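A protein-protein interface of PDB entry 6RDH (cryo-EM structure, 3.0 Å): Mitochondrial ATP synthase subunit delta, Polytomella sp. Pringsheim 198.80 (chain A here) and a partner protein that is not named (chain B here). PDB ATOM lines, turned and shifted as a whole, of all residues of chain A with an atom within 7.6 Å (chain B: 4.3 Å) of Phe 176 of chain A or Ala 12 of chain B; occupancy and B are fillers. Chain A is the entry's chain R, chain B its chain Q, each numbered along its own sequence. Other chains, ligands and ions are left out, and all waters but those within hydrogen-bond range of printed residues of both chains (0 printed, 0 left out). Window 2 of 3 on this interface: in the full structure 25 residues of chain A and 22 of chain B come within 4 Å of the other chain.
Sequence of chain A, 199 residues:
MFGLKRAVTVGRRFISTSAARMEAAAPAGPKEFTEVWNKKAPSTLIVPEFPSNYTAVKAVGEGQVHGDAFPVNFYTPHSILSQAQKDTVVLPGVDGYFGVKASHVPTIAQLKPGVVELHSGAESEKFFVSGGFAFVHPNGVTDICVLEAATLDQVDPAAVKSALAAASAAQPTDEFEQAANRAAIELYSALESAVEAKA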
ATOM      1  N   PRO A 172     -21.792  19.832  16.209  1.00  0.00           N
ATOM      2  CA  PRO A 172     -20.985  19.961  17.428  1.00  0.00           C
ATOM      3  C   PRO A 172     -21.837  19.952  18.687  1.00  0.00           C
ATOM      4  O   PRO A 172     -23.049  19.722  18.624  1.00  0.00           O
ATOM      5  CB  PRO A 172     -20.283  21.309  17.234  1.00  0.00           C
ATOM      6  CG  PRO A 172     -21.234  22.094  16.408  1.00  0.00           C
ATOM      7  CD  PRO A 172     -21.897  21.109  15.483  1.00  0.00           C
ATOM      8  N   THR A 173     -21.217  20.214  19.836  1.00  0.00           N
ATOM      9  CA  THR A 173     -21.932  20.277  21.106  1.00  0.00           C
ATOM     10  C   THR A 173     -22.694  21.585  21.300  1.00  0.00           C
ATOM     11  O   THR A 173     -23.351  21.750  22.335  1.00  0.00           O
ATOM     12  CB  THR A 173     -20.960  20.070  22.271  1.00  0.00           C
ATOM     13  OG1 THR A 173     -20.059  21.183  22.351  1.00  0.00           O
ATOM     14  CG2 THR A 173     -20.168  18.787  22.083  1.00  0.00           C
ATOM     15  N   ASP A 174     -22.608  22.511  20.348  1.00  0.00           N
ATOM     16  CA  ASP A 174     -23.421  23.717  20.382  1.00  0.00           C
ATOM     17  C   ASP A 174     -24.892  23.362  20.223  1.00  0.00           C
ATOM     18  O   ASP A 174     -25.254  22.535  19.390  1.00  0.00           O
ATOM     19  CB  ASP A 174     -22.997  24.662  19.262  1.00  0.00           C
ATOM     20  CG  ASP A 174     -23.382  26.100  19.526  1.00  0.00           C
ATOM     21  OD1 ASP A 174     -24.129  26.358  20.492  1.00  0.00           O
ATOM     22  OD2 ASP A 174     -22.946  26.978  18.753  1.00  0.00           O
ATOM     23  N   GLU A 175     -25.741  24.000  21.017  1.00  0.00           N
ATOM     24  CA  GLU A 175     -27.177  23.865  20.827  1.00  0.00           C
ATOM     25  C   GLU A 175     -27.683  24.807  19.746  1.00  0.00           C
ATOM     26  O   GLU A 175     -28.689  24.516  19.082  1.00  0.00           O
ATOM     27  CB  GLU A 175     -27.905  24.128  22.149  1.00  0.00           C
ATOM     28  CG  GLU A 175     -27.675  25.515  22.735  1.00  0.00           C
ATOM     29  CD  GLU A 175     -28.360  25.715  24.070  1.00  0.00           C
ATOM     30  OE1 GLU A 175     -29.015  24.763  24.549  1.00  0.00           O
ATOM     31  OE2 GLU A 175     -28.248  26.822  24.639  1.00  0.00           O
ATOM     32  N   PHE A 176     -26.955  25.903  19.535  1.00  0.00           N
ATOM     33  CA  PHE A 176     -27.317  26.890  18.532  1.00  0.00           C
ATOM     34  C   PHE A 176     -27.159  26.307  17.134  1.00  0.00           C
ATOM     35  O   PHE A 176     -28.040  26.454  16.279  1.00  0.00           O
ATOM     36  CB  PHE A 176     -26.427  28.111  18.705  1.00  0.00           C
ATOM     37  CG  PHE A 176     -27.023  29.373  18.205  1.00  0.00           C
ATOM     38  CD1 PHE A 176     -27.803  30.144  19.049  1.00  0.00           C
ATOM     39  CD2 PHE A 176     -26.843  29.783  16.900  1.00  0.00           C
ATOM     40  CE1 PHE A 176     -28.353  31.320  18.616  1.00  0.00           C
ATOM     41  CE2 PHE A 176     -27.403  30.957  16.455  1.00  0.00           C
ATOM     42  CZ  PHE A 176     -28.157  31.720  17.319  1.00  0.00           C
ATOM     43  N   GLU A 177     -26.046  25.612  16.895  1.00  0.00           N
ATOM     44  CA  GLU A 177     -25.861  24.961  15.609  1.00  0.00           C
ATOM     45  C   GLU A 177     -26.741  23.735  15.458  1.00  0.00           C
ATOM     46  O   GLU A 177     -27.063  23.383  14.326  1.00  0.00           O
ATOM     47  CB  GLU A 177     -24.400  24.578  15.383  1.00  0.00           C
ATOM     48  CG  GLU A 177     -23.991  24.582  13.904  1.00  0.00           C
ATOM     49  CD  GLU A 177     -24.166  23.232  13.202  1.00  0.00           C
ATOM     50  OE1 GLU A 177     -24.483  22.226  13.869  1.00  0.00           O
ATOM     51  OE2 GLU A 177     -23.994  23.180  11.968  1.00  0.00           O
ATOM     52  N   GLN A 178     -27.158  23.090  16.554  1.00  0.00           N
ATOM     53  CA  GLN A 178     -28.185  22.056  16.433  1.00  0.00           C
ATOM     54  C   GLN A 178     -29.490  22.637  15.922  1.00  0.00           C
ATOM     55  O   GLN A 178     -30.134  22.047  15.048  1.00  0.00           O
ATOM     56  CB  GLN A 178     -28.433  21.341  17.762  1.00  0.00           C
ATOM     57  CG  GLN A 178     -27.331  20.421  18.235  1.00  0.00           C
ATOM     58  CD  GLN A 178     -27.171  19.183  17.382  1.00  0.00           C
ATOM     59  OE1 GLN A 178     -26.068  18.650  17.252  1.00  0.00           O
ATOM     60  NE2 GLN A 178     -28.270  18.705  16.808  1.00  0.00           N
ATOM     61  N   ALA A 179     -29.873  23.810  16.427  1.00  0.00           N
ATOM     62  CA  ALA A 179     -31.096  24.446  15.946  1.00  0.00           C
ATOM     63  C   ALA A 179     -30.961  24.891  14.493  1.00  0.00           C
ATOM     64  O   ALA A 179     -31.859  24.639  13.678  1.00  0.00           O
ATOM     65  CB  ALA A 179     -31.451  25.623  16.848  1.00  0.00           C
ATOM     66  N   ALA A 180     -29.831  25.517  14.146  1.00  0.00           N
ATOM     67  CA  ALA A 180     -29.611  25.976  12.777  1.00  0.00           C
ATOM     68  C   ALA A 180     -29.479  24.816  11.802  1.00  0.00           C
ATOM     69  O   ALA A 180     -29.974  24.893  10.673  1.00  0.00           O
ATOM     70  CB  ALA A 180     -28.367  26.857  12.713  1.00  0.00           C
ATOM     71  N   ASN A 181     -28.880  23.714  12.240  1.00  0.00           N
ATOM     72  CA  ASN A 181     -28.727  22.541  11.398  1.00  0.00           C
ATOM     73  C   ASN A 181     -30.044  21.786  11.244  1.00  0.00           C
ATOM     74  O   ASN A 181     -30.310  21.213  10.184  1.00  0.00           O
ATOM     75  CB  ASN A 181     -27.640  21.652  11.994  1.00  0.00           C
ATOM     76  CG  ASN A 181     -27.356  20.447  11.159  1.00  0.00           C
ATOM     77  OD1 ASN A 181     -27.328  19.325  11.658  1.00  0.00           O
ATOM     78  ND2 ASN A 181     -27.148  20.662   9.870  1.00  0.00           N
ATOM     79  N   ARG A 182     -30.892  21.794  12.279  1.00  0.00           N
ATOM     80  CA  ARG A 182     -32.217  21.195  12.151  1.00  0.00           C
ATOM     81  C   ARG A 182     -33.090  21.999  11.201  1.00  0.00           C
ATOM     82  O   ARG A 182     -33.815  21.424  10.377  1.00  0.00           O
ATOM     83  CB  ARG A 182     -32.886  21.083  13.520  1.00  0.00           C
ATOM     84  CG  ARG A 182     -34.295  20.518  13.463  1.00  0.00           C
ATOM     85  CD  ARG A 182     -34.875  20.301  14.836  1.00  0.00           C
ATOM     86  NE  ARG A 182     -36.302  20.015  14.768  1.00  0.00           N
ATOM     87  CZ  ARG A 182     -37.061  19.763  15.825  1.00  0.00           C
ATOM     88  NH1 ARG A 182     -36.528  19.761  17.035  1.00  0.00           N
ATOM     89  NH2 ARG A 182     -38.353  19.518  15.672  1.00  0.00           N
ATOM     90  N   PHE B   8     -37.954  24.649  19.087  1.00  0.00           N
ATOM     91  CA  PHE B   8     -36.567  24.203  19.196  1.00  0.00           C
ATOM     92  C   PHE B   8     -35.572  25.337  19.002  1.00  0.00           C
ATOM     93  O   PHE B   8     -34.450  25.263  19.511  1.00  0.00           O
ATOM     94  CB  PHE B   8     -36.290  23.075  18.201  1.00  0.00           C
ATOM     95  CG  PHE B   8     -36.326  23.493  16.759  1.00  0.00           C
ATOM     96  CD1 PHE B   8     -35.156  23.781  16.075  1.00  0.00           C
ATOM     97  CD2 PHE B   8     -37.521  23.544  16.071  1.00  0.00           C
ATOM     98  CE1 PHE B   8     -35.186  24.153  14.755  1.00  0.00           C
ATOM     99  CE2 PHE B   8     -37.555  23.911  14.747  1.00  0.00           C
ATOM    100  CZ  PHE B   8     -36.385  24.211  14.089  1.00  0.00           C
ATOM    101  N   TYR B   9     -35.950  26.383  18.274  1.00  0.00           N
ATOM    102  CA  TYR B   9     -35.097  27.560  18.220  1.00  0.00           C
ATOM    103  C   TYR B   9     -35.140  28.325  19.531  1.00  0.00           C
ATOM    104  O   TYR B   9     -34.125  28.881  19.954  1.00  0.00           O
ATOM    105  CB  TYR B   9     -35.501  28.462  17.056  1.00  0.00           C
ATOM    106  CG  TYR B   9     -36.982  28.692  16.903  1.00  0.00           C
ATOM    107  CD1 TYR B   9     -37.737  27.909  16.047  1.00  0.00           C
ATOM    108  CD2 TYR B   9     -37.619  29.713  17.587  1.00  0.00           C
ATOM    109  CE1 TYR B   9     -39.080  28.120  15.897  1.00  0.00           C
ATOM    110  CE2 TYR B   9     -38.962  29.930  17.442  1.00  0.00           C
ATOM    111  CZ  TYR B   9     -39.686  29.132  16.597  1.00  0.00           C
ATOM    112  OH  TYR B   9     -41.030  29.344  16.446  1.00  0.00           O
ATOM    113  N   ARG B  10     -36.290  28.342  20.201  1.00  0.00           N
ATOM    114  CA  ARG B  10     -36.409  29.067  21.456  1.00  0.00           C
ATOM    115  C   ARG B  10     -35.683  28.355  22.585  1.00  0.00           C
ATOM    116  O   ARG B  10     -35.158  29.011  23.488  1.00  0.00           O
ATOM    117  CB  ARG B  10     -37.882  29.252  21.800  1.00  0.00           C
ATOM    118  CG  ARG B  10     -38.147  30.252  22.882  1.00  0.00           C
ATOM    119  CD  ARG B  10     -37.803  31.645  22.416  1.00  0.00           C
ATOM    120  NE  ARG B  10     -38.615  32.062  21.281  1.00  0.00           N
ATOM    121  CZ  ARG B  10     -38.682  33.313  20.845  1.00  0.00           C
ATOM    122  NH1 ARG B  10     -37.990  34.262  21.455  1.00  0.00           N
ATOM    123  NH2 ARG B  10     -39.444  33.619  19.811  1.00  0.00           N
ATOM    124  N   VAL B  11     -35.643  27.020  22.551  1.00  0.00           N
ATOM    125  CA  VAL B  11     -34.898  26.265  23.553  1.00  0.00           C
ATOM    126  C   VAL B  11     -33.404  26.498  23.400  1.00  0.00           C
ATOM    127  O   VAL B  11     -32.682  26.623  24.396  1.00  0.00           O
ATOM    128  CB  VAL B  11     -35.247  24.767  23.472  1.00  0.00           C
ATOM    129  CG1 VAL B  11     -34.632  24.012  24.629  1.00  0.00           C
ATOM    130  CG2 VAL B  11     -36.738  24.582  23.518  1.00  0.00           C
ATOM    131  N   ALA B  12     -32.920  26.612  22.169  1.00  0.00           N
ATOM    132  CA  ALA B  12     -31.503  26.836  21.924  1.00  0.00           C
ATOM    133  C   ALA B  12     -31.092  28.295  22.052  1.00  0.00           C
ATOM    134  O   ALA B  12     -30.029  28.663  21.544  1.00  0.00           O
ATOM    135  CB  ALA B  12     -31.125  26.319  20.537  1.00  0.00           C
ATOM    136  N   GLY B  13     -31.901  29.139  22.695  1.00  0.00           N
ATOM    137  CA  GLY B  13     -31.582  30.536  22.882  1.00  0.00           C
ATOM    138  C   GLY B  13     -31.809  31.418  21.678  1.00  0.00           C
ATOM    139  O   GLY B  13     -31.704  32.643  21.802  1.00  0.00           O
ATOM    140  N   MET B  14     -32.122  30.844  20.525  1.00  0.00           N
ATOM    141  CA  MET B  14     -32.278  31.608  19.302  1.00  0.00           C
ATOM    142  C   MET B  14     -33.631  32.300  19.288  1.00  0.00           C
ATOM    143  O   MET B  14     -34.631  31.748  19.747  1.00  0.00           O
ATOM    144  CB  MET B  14     -32.135  30.677  18.101  1.00  0.00           C
ATOM    145  CG  MET B  14     -31.949  31.356  16.783  1.00  0.00           C
ATOM    146  SD  MET B  14     -31.845  30.142  15.471  1.00  0.00           S
ATOM    147  CE  MET B  14     -30.536  29.124  16.093  1.00  0.00           C
ATOM    148  N   ARG B  18     -34.046  35.419  14.197  1.00  0.00           N
ATOM    149  CA  ARG B  18     -32.796  34.854  13.723  1.00  0.00           C
ATOM    150  C   ARG B  18     -33.016  33.496  13.090  1.00  0.00           C
ATOM    151  O   ARG B  18     -32.374  33.167  12.092  1.00  0.00           O
ATOM    152  CB  ARG B  18     -31.790  34.747  14.855  1.00  0.00           C
ATOM    153  CG  ARG B  18     -30.401  34.516  14.334  1.00  0.00           C
ATOM    154  CD  ARG B  18     -29.420  34.388  15.447  1.00  0.00           C
ATOM    155  NE  ARG B  18     -29.203  35.628  16.168  1.00  0.00           N
ATOM    156  CZ  ARG B  18     -28.270  36.507  15.842  1.00  0.00           C
ATOM    157  NH1 ARG B  18     -27.481  36.273  14.807  1.00  0.00           N
ATOM    158  NH2 ARG B  18     -28.124  37.615  16.550  1.00  0.00           N
ATOM    159  N   LYS B  71     -25.192  32.412  11.501  1.00  0.00           N
ATOM    160  CA  LYS B  71     -25.698  31.084  11.829  1.00  0.00           C
ATOM    161  C   LYS B  71     -25.247  30.637  13.209  1.00  0.00           C
ATOM    162  O   LYS B  71     -25.944  29.857  13.864  1.00  0.00           O
ATOM    163  CB  LYS B  71     -25.235  30.060  10.797  1.00  0.00           C
ATOM    164  CG  LYS B  71     -25.689  30.294   9.369  1.00  0.00           C
ATOM    165  CD  LYS B  71     -24.774  29.528   8.423  1.00  0.00           C
ATOM    166  CE  LYS B  71     -25.418  29.246   7.081  1.00  0.00           C
ATOM    167  NZ  LYS B  71     -25.872  30.475   6.381  1.00  0.00           N
ATOM    168  N   THR B  72     -24.077  31.086  13.648  1.00  0.00           N
ATOM    169  CA  THR B  72     -23.529  30.694  14.932  1.00  0.00           C
ATOM    170  C   THR B  72     -24.043  31.662  16.006  1.00  0.00           C
ATOM    171  O   THR B  72     -24.658  32.685  15.702  1.00  0.00           O
ATOM    172  CB  THR B  72     -22.003  30.669  14.842  1.00  0.00           C
ATOM    173  OG1 THR B  72     -21.634  30.165  13.553  1.00  0.00           O
ATOM    174  CG2 THR B  72     -21.394  29.692  15.841  1.00  0.00           C
ATOM    175  N   ALA B  73     -23.802  31.321  17.272  1.00  0.00           N
ATOM    176  CA  ALA B  73     -24.392  32.012  18.410  1.00  0.00           C
ATOM    177  C   ALA B  73     -23.856  33.429  18.569  1.00  0.00           C
ATOM    178  O   ALA B  73     -22.846  33.817  17.979  1.00  0.00           O
ATOM    179  CB  ALA B  73     -24.129  31.230  19.695  1.00  0.00           C
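Of the 11 printed residues of chain A, 4 touch a printed residue of chain B.
The backbone NH (N) of Met 14 of chain B is in hydrogen-bond range of the backbone carbonyl oxygen (O) of Tyr 9 of chain B, 2.9 Å away. N of Phe 176 of chain A sits at hydrogen-bond distance from OD1 of Asp 174 of chain A, at 3.0 Å.
Of chain B, only Ala 12, Met 14, Arg 18, Lys 71, Thr 72 and Ala 73 come within 4 Å of Phe 176 of chain A. Ala 12 of chain B touches just these residues of chain A: Glu 175, Phe 176 and Ala 179. Of the printed residues of chain A, Phe 8 of chain B touches Ala 179 and Arg 182. Printed residues of chain A within 4 Å of Met 14 of chain B: Phe 176 and Ala 179. Printed residues of chain B within 4 Å of Ala 179 of chain A: Phe 8, Ala 12 and Met 14. Of the printed residues of chain A, Thr 72 of chain B touches Phe 176. Printed residues of chain B within 4 Å of Glu 175 of chain A: Ala 12. Ala 180 of chain A touches none of the printed residues of chain B. Tyr 9 of chain B touches none of the printed residues of chain A. The nearest printed residue of chain B that does not touch Phe 176 of chain A is Gly 13 of chain B (4.6 Å). The nearest residue of chain A that does not touch Ala 12 of chain B is Gln 178 of chain A (6.1 Å).
Among the printed residues, merely in contact across the chains: Glu 175 of chain A with Ala 12 of chain B, Phe 176 of chain A with Ala 12 of chain B, Phe 176 of chain A with Met 14 of chain B, Phe 176 of chain A with Arg 18 of chain B, Phe 176 of chain A with Lys 71 of chain B, Phe 176 of chain A with Thr 72 of chain B, Phe 176 of chain A with Ala 73 of chain B, Ala 179 of chain A with Phe 8 of chain B, Ala 179 of chain A with Ala 12 of chain B, Ala 179 of chain A with Met 14 of chain B and Arg 182 of chain A with Phe 8 of chain B.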
